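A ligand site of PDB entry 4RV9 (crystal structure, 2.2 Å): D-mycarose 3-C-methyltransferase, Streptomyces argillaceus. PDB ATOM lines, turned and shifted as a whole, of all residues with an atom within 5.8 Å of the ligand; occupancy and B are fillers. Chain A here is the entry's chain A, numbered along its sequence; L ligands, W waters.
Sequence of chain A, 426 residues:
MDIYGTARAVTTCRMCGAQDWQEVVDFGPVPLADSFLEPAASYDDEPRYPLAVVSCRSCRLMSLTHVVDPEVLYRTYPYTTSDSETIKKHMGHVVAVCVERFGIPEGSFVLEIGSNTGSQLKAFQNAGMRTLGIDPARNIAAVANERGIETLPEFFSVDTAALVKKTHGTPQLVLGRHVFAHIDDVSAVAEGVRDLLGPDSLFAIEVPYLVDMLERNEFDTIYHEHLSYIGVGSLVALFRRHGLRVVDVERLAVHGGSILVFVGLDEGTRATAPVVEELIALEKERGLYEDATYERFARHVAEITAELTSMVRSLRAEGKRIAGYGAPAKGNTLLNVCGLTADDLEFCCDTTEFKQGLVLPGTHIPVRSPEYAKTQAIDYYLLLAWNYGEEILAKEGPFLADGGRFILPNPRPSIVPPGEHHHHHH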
ATOM      1  N   TYR A  74      31.159  11.985  18.481  1.00  0.00           N
ATOM      2  CA  TYR A  74      31.186  10.585  18.937  1.00  0.00           C
ATOM      3  C   TYR A  74      31.924   9.583  18.051  1.00  0.00           C
ATOM      4  O   TYR A  74      32.319   8.523  18.539  1.00  0.00           O
ATOM      5  CB  TYR A  74      29.758  10.104  19.227  1.00  0.00           C
ATOM      6  CG  TYR A  74      29.090  10.967  20.260  1.00  0.00           C
ATOM      7  CD1 TYR A  74      29.617  11.088  21.537  1.00  0.00           C
ATOM      8  CD2 TYR A  74      27.946  11.696  19.955  1.00  0.00           C
ATOM      9  CE1 TYR A  74      29.031  11.893  22.490  1.00  0.00           C
ATOM     10  CE2 TYR A  74      27.353  12.514  20.905  1.00  0.00           C
ATOM     11  CZ  TYR A  74      27.896  12.608  22.171  1.00  0.00           C
ATOM     12  OH  TYR A  74      27.317  13.426  23.123  1.00  0.00           O
ATOM     13  N   TYR A  77      35.554   8.874  19.885  1.00  0.00           N
ATOM     14  CA  TYR A  77      35.372   9.316  21.270  1.00  0.00           C
ATOM     15  C   TYR A  77      36.530   8.766  22.105  1.00  0.00           C
ATOM     16  O   TYR A  77      36.957   7.635  21.900  1.00  0.00           O
ATOM     17  CB  TYR A  77      34.038   8.810  21.801  1.00  0.00           C
ATOM     18  CG  TYR A  77      33.488   9.550  23.002  1.00  0.00           C
ATOM     19  CD1 TYR A  77      33.128  10.895  22.914  1.00  0.00           C
ATOM     20  CD2 TYR A  77      33.281   8.882  24.213  1.00  0.00           C
ATOM     21  CE1 TYR A  77      32.612  11.562  24.015  1.00  0.00           C
ATOM     22  CE2 TYR A  77      32.766   9.540  25.310  1.00  0.00           C
ATOM     23  CZ  TYR A  77      32.436  10.881  25.208  1.00  0.00           C
ATOM     24  OH  TYR A  77      31.915  11.533  26.293  1.00  0.00           O
ATOM     25  N   MET A  91      28.224  -0.357  38.294  1.00  0.00           N
ATOM     26  CA  MET A  91      27.773  -1.216  37.204  1.00  0.00           C
ATOM     27  C   MET A  91      27.179  -2.535  37.725  1.00  0.00           C
ATOM     28  O   MET A  91      26.198  -3.043  37.168  1.00  0.00           O
ATOM     29  CB  MET A  91      28.909  -1.498  36.221  1.00  0.00           C
ATOM     30  CG  MET A  91      29.278  -0.325  35.329  1.00  0.00           C
ATOM     31  SD  MET A  91      30.484  -0.812  34.080  1.00  0.00           S
ATOM     32  CE  MET A  91      30.663   0.726  33.178  1.00  0.00           C
ATOM     33  N   GLU A 112      22.333  -2.901  25.127  1.00  0.00           N
ATOM     34  CA  GLU A 112      22.788  -1.616  25.686  1.00  0.00           C
ATOM     35  C   GLU A 112      23.151  -0.584  24.619  1.00  0.00           C
ATOM     36  O   GLU A 112      23.976  -0.845  23.737  1.00  0.00           O
ATOM     37  CB  GLU A 112      23.962  -1.813  26.645  1.00  0.00           C
ATOM     38  CG  GLU A 112      24.410  -0.491  27.266  1.00  0.00           C
ATOM     39  CD  GLU A 112      25.535  -0.637  28.274  1.00  0.00           C
ATOM     40  OE1 GLU A 112      25.832   0.352  28.954  1.00  0.00           O
ATOM     41  OE2 GLU A 112      26.119  -1.734  28.359  1.00  0.00           O
ATOM     42  N   ILE A 113      22.534   0.582  24.742  1.00  0.00           N
ATOM     43  CA  ILE A 113      22.800   1.722  23.885  1.00  0.00           C
ATOM     44  C   ILE A 113      23.892   2.556  24.541  1.00  0.00           C
ATOM     45  O   ILE A 113      23.808   2.890  25.716  1.00  0.00           O
ATOM     46  CB  ILE A 113      21.515   2.584  23.727  1.00  0.00           C
ATOM     47  CG1 ILE A 113      20.429   1.774  23.020  1.00  0.00           C
ATOM     48  CG2 ILE A 113      21.814   3.852  22.932  1.00  0.00           C
ATOM     49  CD1 ILE A 113      19.041   2.397  23.108  1.00  0.00           C
ATOM     50  N   GLY A 114      24.914   2.927  23.774  1.00  0.00           N
ATOM     51  CA  GLY A 114      26.044   3.676  24.308  1.00  0.00           C
ATOM     52  C   GLY A 114      26.909   2.809  25.193  1.00  0.00           C
ATOM     53  O   GLY A 114      27.447   3.270  26.204  1.00  0.00           O
ATOM     54  N   SER A 115      27.064   1.547  24.774  1.00  0.00           N
ATOM     55  CA  SER A 115      27.754   0.514  25.540  1.00  0.00           C
ATOM     56  C   SER A 115      29.277   0.722  25.698  1.00  0.00           C
ATOM     57  O   SER A 115      29.908   0.087  26.546  1.00  0.00           O
ATOM     58  CB  SER A 115      27.486  -0.872  24.916  1.00  0.00           C
ATOM     59  OG  SER A 115      27.865  -0.924  23.551  1.00  0.00           O
ATOM     60  N   ASN A 116      29.849   1.604  24.874  1.00  0.00           N
ATOM     61  CA  ASN A 116      31.227   2.053  25.088  1.00  0.00           C
ATOM     62  C   ASN A 116      32.180   0.836  25.080  1.00  0.00           C
ATOM     63  O   ASN A 116      32.063  -0.021  24.183  1.00  0.00           O
ATOM     64  CB  ASN A 116      31.290   2.861  26.402  1.00  0.00           C
ATOM     65  CG  ASN A 116      32.517   3.761  26.493  1.00  0.00           C
ATOM     66  OD1 ASN A 116      33.545   3.350  27.025  1.00  0.00           O
ATOM     67  ND2 ASN A 116      32.417   4.973  25.958  1.00  0.00           N
ATOM     68  N   ILE A 134      25.476  -1.256  21.289  1.00  0.00           N
ATOM     69  CA  ILE A 134      25.362  -0.322  20.173  1.00  0.00           C
ATOM     70  C   ILE A 134      26.091   0.949  20.583  1.00  0.00           C
ATOM     71  O   ILE A 134      25.704   1.577  21.570  1.00  0.00           O
ATOM     72  CB  ILE A 134      23.899   0.022  19.844  1.00  0.00           C
ATOM     73  CG1 ILE A 134      23.147  -1.217  19.383  1.00  0.00           C
ATOM     74  CG2 ILE A 134      23.805   1.108  18.783  1.00  0.00           C
ATOM     75  CD1 ILE A 134      21.640  -1.043  19.402  1.00  0.00           C
ATOM     76  N   ASP A 135      27.145   1.306  19.852  1.00  0.00           N
ATOM     77  CA  ASP A 135      27.926   2.507  20.134  1.00  0.00           C
ATOM     78  C   ASP A 135      28.627   3.004  18.866  1.00  0.00           C
ATOM     79  O   ASP A 135      29.353   2.239  18.236  1.00  0.00           O
ATOM     80  CB  ASP A 135      28.956   2.256  21.240  1.00  0.00           C
ATOM     81  CG  ASP A 135      29.475   3.527  21.862  1.00  0.00           C
ATOM     82  OD1 ASP A 135      29.289   3.727  23.074  1.00  0.00           O
ATOM     83  OD2 ASP A 135      30.064   4.363  21.143  1.00  0.00           O
ATOM     84  N   PRO A 136      28.414   4.277  18.496  1.00  0.00           N
ATOM     85  CA  PRO A 136      28.948   4.823  17.241  1.00  0.00           C
ATOM     86  C   PRO A 136      30.468   5.071  17.237  1.00  0.00           C
ATOM     87  O   PRO A 136      31.047   5.201  16.156  1.00  0.00           O
ATOM     88  CB  PRO A 136      28.203   6.155  17.097  1.00  0.00           C
ATOM     89  CG  PRO A 136      27.935   6.574  18.494  1.00  0.00           C
ATOM     90  CD  PRO A 136      27.642   5.296  19.238  1.00  0.00           C
ATOM     91  N   ALA A 137      31.079   5.155  18.412  1.00  0.00           N
ATOM     92  CA  ALA A 137      32.522   5.404  18.518  1.00  0.00           C
ATOM     93  C   ALA A 137      33.305   4.192  18.009  1.00  0.00           C
ATOM     94  O   ALA A 137      33.447   3.183  18.711  1.00  0.00           O
ATOM     95  CB  ALA A 137      32.907   5.734  19.944  1.00  0.00           C
ATOM     96  N   ILE A 140      36.237   2.782  20.002  1.00  0.00           N
ATOM     97  CA  ILE A 140      35.835   2.132  21.239  1.00  0.00           C
ATOM     98  C   ILE A 140      35.149   0.809  20.951  1.00  0.00           C
ATOM     99  O   ILE A 140      35.383  -0.172  21.652  1.00  0.00           O
ATOM    100  CB  ILE A 140      34.920   3.039  22.063  1.00  0.00           C
ATOM    101  CG1 ILE A 140      35.731   4.235  22.580  1.00  0.00           C
ATOM    102  CG2 ILE A 140      34.313   2.271  23.240  1.00  0.00           C
ATOM    103  CD1 ILE A 140      34.889   5.378  23.113  1.00  0.00           C
ATOM    104  N   GLU A 154      27.318   1.702  15.528  1.00  0.00           N
ATOM    105  CA  GLU A 154      26.336   2.617  14.958  1.00  0.00           C
ATOM    106  C   GLU A 154      25.621   3.432  16.042  1.00  0.00           C
ATOM    107  O   GLU A 154      25.647   3.077  17.226  1.00  0.00           O
ATOM    108  CB  GLU A 154      25.282   1.856  14.145  1.00  0.00           C
ATOM    109  CG  GLU A 154      25.848   0.999  13.009  1.00  0.00           C
ATOM    110  CD  GLU A 154      26.606   1.784  11.942  1.00  0.00           C
ATOM    111  OE1 GLU A 154      26.572   3.038  11.933  1.00  0.00           O
ATOM    112  OE2 GLU A 154      27.243   1.140  11.076  1.00  0.00           O
ATOM    113  N   PHE A 155      24.998   4.526  15.616  1.00  0.00           N
ATOM    114  CA  PHE A 155      24.070   5.262  16.453  1.00  0.00           C
ATOM    115  C   PHE A 155      22.810   4.431  16.570  1.00  0.00           C
ATOM    116  O   PHE A 155      22.487   3.676  15.659  1.00  0.00           O
ATOM    117  CB  PHE A 155      23.719   6.628  15.853  1.00  0.00           C
ATOM    118  CG  PHE A 155      24.857   7.601  15.842  1.00  0.00           C
ATOM    119  CD1 PHE A 155      25.069   8.465  16.908  1.00  0.00           C
ATOM    120  CD2 PHE A 155      25.728   7.660  14.768  1.00  0.00           C
ATOM    121  CE1 PHE A 155      26.122   9.358  16.915  1.00  0.00           C
ATOM    122  CE2 PHE A 155      26.776   8.561  14.754  1.00  0.00           C
ATOM    123  CZ  PHE A 155      26.972   9.410  15.828  1.00  0.00           C
ATOM    124  N   PHE A 156      22.129   4.532  17.707  1.00  0.00           N
ATOM    125  CA  PHE A 156      20.835   3.873  17.852  1.00  0.00           C
ATOM    126  C   PHE A 156      19.832   4.651  16.997  1.00  0.00           C
ATOM    127  O   PHE A 156      19.870   5.871  16.926  1.00  0.00           O
ATOM    128  CB  PHE A 156      20.382   3.847  19.306  1.00  0.00           C
ATOM    129  CG  PHE A 156      19.088   3.114  19.519  1.00  0.00           C
ATOM    130  CD1 PHE A 156      19.040   1.734  19.453  1.00  0.00           C
ATOM    131  CD2 PHE A 156      17.909   3.809  19.772  1.00  0.00           C
ATOM    132  CE1 PHE A 156      17.840   1.050  19.644  1.00  0.00           C
ATOM    133  CE2 PHE A 156      16.702   3.137  19.959  1.00  0.00           C
ATOM    134  CZ  PHE A 156      16.675   1.746  19.898  1.00  0.00           C
ATOM    135  N   ARG A 177      22.880   4.087  29.631  1.00  0.00           N
ATOM    136  CA  ARG A 177      23.520   4.744  30.782  1.00  0.00           C
ATOM    137  C   ARG A 177      24.167   6.044  30.360  1.00  0.00           C
ATOM    138  O   ARG A 177      25.162   6.032  29.634  1.00  0.00           O
ATOM    139  CB  ARG A 177      24.551   3.825  31.419  1.00  0.00           C
ATOM    140  CG  ARG A 177      23.944   2.670  32.208  1.00  0.00           C
ATOM    141  CD  ARG A 177      24.905   2.149  33.269  1.00  0.00           C
ATOM    142  NE  ARG A 177      25.369   3.207  34.162  1.00  0.00           N
ATOM    143  CZ  ARG A 177      26.632   3.658  34.255  1.00  0.00           C
ATOM    144  NH1 ARG A 177      27.615   3.133  33.519  1.00  0.00           N
ATOM    145  NH2 ARG A 177      26.903   4.649  35.097  1.00  0.00           N
ATOM    146  N   HIS A 178      23.573   7.152  30.787  1.00  0.00           N
ATOM    147  CA  HIS A 178      24.017   8.529  30.504  1.00  0.00           C
ATOM    148  C   HIS A 178      23.783   9.016  29.068  1.00  0.00           C
ATOM    149  O   HIS A 178      23.461  10.199  28.856  1.00  0.00           O
ATOM    150  CB  HIS A 178      25.434   8.778  31.021  1.00  0.00           C
ATOM    151  CG  HIS A 178      25.505   8.705  32.511  1.00  0.00           C
ATOM    152  ND1 HIS A 178      25.438   9.839  33.303  1.00  0.00           N
ATOM    153  CD2 HIS A 178      25.532   7.657  33.355  1.00  0.00           C
ATOM    154  CE1 HIS A 178      25.453   9.476  34.576  1.00  0.00           C
ATOM    155  NE2 HIS A 178      25.525   8.148  34.633  1.00  0.00           N
ATOM    156  N   VAL A 179      23.894   8.101  28.115  1.00  0.00           N
ATOM    157  CA  VAL A 179      23.719   8.375  26.698  1.00  0.00           C
ATOM    158  C   VAL A 179      22.418   9.098  26.333  1.00  0.00           C
ATOM    159  O   VAL A 179      22.400   9.882  25.393  1.00  0.00           O
ATOM    160  CB  VAL A 179      23.842   7.073  25.874  1.00  0.00           C
ATOM    161  CG1 VAL A 179      22.685   6.114  26.170  1.00  0.00           C
ATOM    162  CG2 VAL A 179      23.931   7.374  24.388  1.00  0.00           C
ATOM    163  N   HIS A 182      22.492  12.647  25.807  1.00  0.00           N
ATOM    164  CA  HIS A 182      23.382  13.028  24.703  1.00  0.00           C
ATOM    165  C   HIS A 182      22.703  12.991  23.316  1.00  0.00           C
ATOM    166  O   HIS A 182      23.324  13.370  22.322  1.00  0.00           O
ATOM    167  CB  HIS A 182      24.600  12.095  24.642  1.00  0.00           C
ATOM    168  CG  HIS A 182      25.509  12.196  25.826  1.00  0.00           C
ATOM    169  ND1 HIS A 182      25.102  11.899  27.107  1.00  0.00           N
ATOM    170  CD2 HIS A 182      26.824  12.518  25.920  1.00  0.00           C
ATOM    171  CE1 HIS A 182      26.113  12.054  27.943  1.00  0.00           C
ATOM    172  NE2 HIS A 182      27.170  12.429  27.245  1.00  0.00           N
ATOM    173  N   ILE A 183      21.457  12.549  23.253  1.00  0.00           N
ATOM    174  CA  ILE A 183      20.770  12.299  21.970  1.00  0.00           C
ATOM    175  C   ILE A 183      19.753  13.393  21.681  1.00  0.00           C
ATOM    176  O   ILE A 183      18.885  13.680  22.499  1.00  0.00           O
ATOM    177  CB  ILE A 183      20.043  10.938  21.980  1.00  0.00           C
ATOM    178  CG1 ILE A 183      21.045   9.813  22.215  1.00  0.00           C
ATOM    179  CG2 ILE A 183      19.317  10.714  20.659  1.00  0.00           C
ATOM    180  CD1 ILE A 183      20.413   8.458  22.519  1.00  0.00           C
ATOM    181  N   GLU A 225      28.022  18.102  24.923  1.00  0.00           N
ATOM    182  CA  GLU A 225      27.566  16.725  24.814  1.00  0.00           C
ATOM    183  C   GLU A 225      26.249  16.512  25.527  1.00  0.00           C
ATOM    184  O   GLU A 225      25.436  15.706  25.095  1.00  0.00           O
ATOM    185  CB  GLU A 225      28.611  15.766  25.395  1.00  0.00           C
ATOM    186  CG  GLU A 225      29.870  15.644  24.561  1.00  0.00           C
ATOM    187  CD  GLU A 225      30.913  14.768  25.203  1.00  0.00           C
ATOM    188  OE1 GLU A 225      30.566  13.707  25.774  1.00  0.00           O
ATOM    189  OE2 GLU A 225      32.098  15.137  25.125  1.00  0.00           O
HETATM  190  N1  LIG L   1      27.587   4.824  28.657  1.00  0.00           N
HETATM  191  C1  LIG L   1      28.849   5.615  28.897  1.00  0.00           C
HETATM  192  C2  LIG L   1      28.577   7.130  29.005  1.00  0.00           C
HETATM  193  C3  LIG L   1      29.183   7.990  27.894  1.00  0.00           C
HETATM  194  S1  LIG L   1      27.898   8.628  26.843  1.00  0.00           S
HETATM  195  C4  LIG L   1      29.488   5.101  30.161  1.00  0.00           C
HETATM  196  O1  LIG L   1      30.614   4.599  30.154  1.00  0.00           O
HETATM  197  O2  LIG L   1      28.879   5.161  31.231  1.00  0.00           O
HETATM  198  C5  LIG L   1      28.681   8.639  25.300  1.00  0.00           C
HETATM  199  C6  LIG L   1      28.766   7.197  24.830  1.00  0.00           C
HETATM  200  O3  LIG L   1      27.563   6.867  24.135  1.00  0.00           O
HETATM  201  C7  LIG L   1      29.920   7.063  23.862  1.00  0.00           C
HETATM  202  O4  LIG L   1      30.484   5.758  23.967  1.00  0.00           O
HETATM  203  C8  LIG L   1      29.227   7.379  22.541  1.00  0.00           C
HETATM  204  O5  LIG L   1      29.900   6.823  21.414  1.00  0.00           O
HETATM  205  C9  LIG L   1      27.847   6.778  22.742  1.00  0.00           C
HETATM  206  N2  LIG L   1      26.748   7.434  21.994  1.00  0.00           N
HETATM  207  C10 LIG L   1      26.574   8.752  21.773  1.00  0.00           C
HETATM  208  N3  LIG L   1      25.436   8.951  21.061  1.00  0.00           N
HETATM  209  C11 LIG L   1      24.869   7.763  20.832  1.00  0.00           C
HETATM  210  C12 LIG L   1      23.660   7.273  20.149  1.00  0.00           C
HETATM  211  N4  LIG L   1      22.810   8.151  19.560  1.00  0.00           N
HETATM  212  N5  LIG L   1      23.427   5.934  20.136  1.00  0.00           N
HETATM  213  C13 LIG L   1      24.277   5.066  20.730  1.00  0.00           C
HETATM  214  N6  LIG L   1      25.399   5.445  21.376  1.00  0.00           N
HETATM  215  C14 LIG L   1      25.739   6.763  21.453  1.00  0.00           C
HETATM  216  O   HOH W   1      20.198   7.698  18.875  1.00  0.00           O
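Water W1 bridges the backbone carbonyl oxygen (O) of Phe 156 (2.7 Å) and a nitrogen (N4) of the ligand (2.7 Å).
The side-chain carboxylate (OE1) of Glu 225 is in hydrogen-bond range of the side-chain hydroxyl (OH) of Tyr 77. The backbone NH of Asn 116 is in hydrogen-bond range of the side-chain carboxylate of Asp 135 (2.8 Å). The backbone carbonyl oxygen of Asp 135 is in hydrogen-bond range of the backbone NH of Glu 154, at 3.4 Å. OD2 of Asp 135 sits at hydrogen-bond distance from N of Ala 137. The side-chain hydroxyl (OG) of Ser 115 sits at hydrogen-bond distance from the backbone NH (N) of Ile 134, at 3.3 Å. O of Glu 112 lies within hydrogen-bond range of N of Ile 134. The backbone carbonyl oxygen (O) of Ile 134 sits at hydrogen-bond distance from the backbone NH (N) of Gly 114 (2.7 Å). ND1 of His 182 sits at hydrogen-bond distance from O of His 178 (2.9 Å).
Tyr 74 touches the ligand (CG to C10, 3.7 Å). Tyr 77 touches the ligand. Ile 113 touches the ligand (CG2 to C13, 3.5 Å). Ile 134 touches the ligand (O to C13, 3.9 Å). CD of Pro 136 touches N6 of the ligand (3.1 Å). Ala 137 touches the ligand. CD1 of Phe 155 touches N4 of the ligand, at 3.5 Å. CG2 of Val 179 touches C14 of the ligand, 3.5 Å away. His 182 touches the ligand (NE2 to S1, 3.9 Å). Ile 183 touches the ligand (CG1 to N4, 3.6 Å). Hydrophobic or aromatic side chains that line the ligand: Tyr 74, Tyr 77, Ile 113, Pro 136, Ala 137, Phe 155, Phe 156, Val 179 and Ile 183. Within 4 Å of the ligand: Tyr 74, Tyr 77, Ile 113, Gly 114, Asn 116, Ile 134, Asp 135, Pro 136, Ala 137, Phe 155, Phe 156, Arg 177, Val 179, His 182 and Ile 183. Along chain A the residues within 4 Å of the ligand span positions 74 to 183.
The guanidinium group of Arg 177 lies within salt-bridge range of an oxygen (O2) of the ligand, at 3.3 Å. ND2 of Asn 116 sits at hydrogen-bond distance from O4 of the ligand (2.9 Å). A nitrogen (N1) of the ligand sits at hydrogen-bond distance from the backbone carbonyl oxygen (O) of Gly 114, 2.9 Å away. O of Arg 177 is in hydrogen-bond range of N1 of the ligand. The backbone NH (N) of Phe 156 lies within hydrogen-bond range of a nitrogen (N5) of the ligand (3.1 Å). The side-chain carboxylate of Asp 135 is in hydrogen-bond range of an oxygen (O5) of the ligand (2.5 Å).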
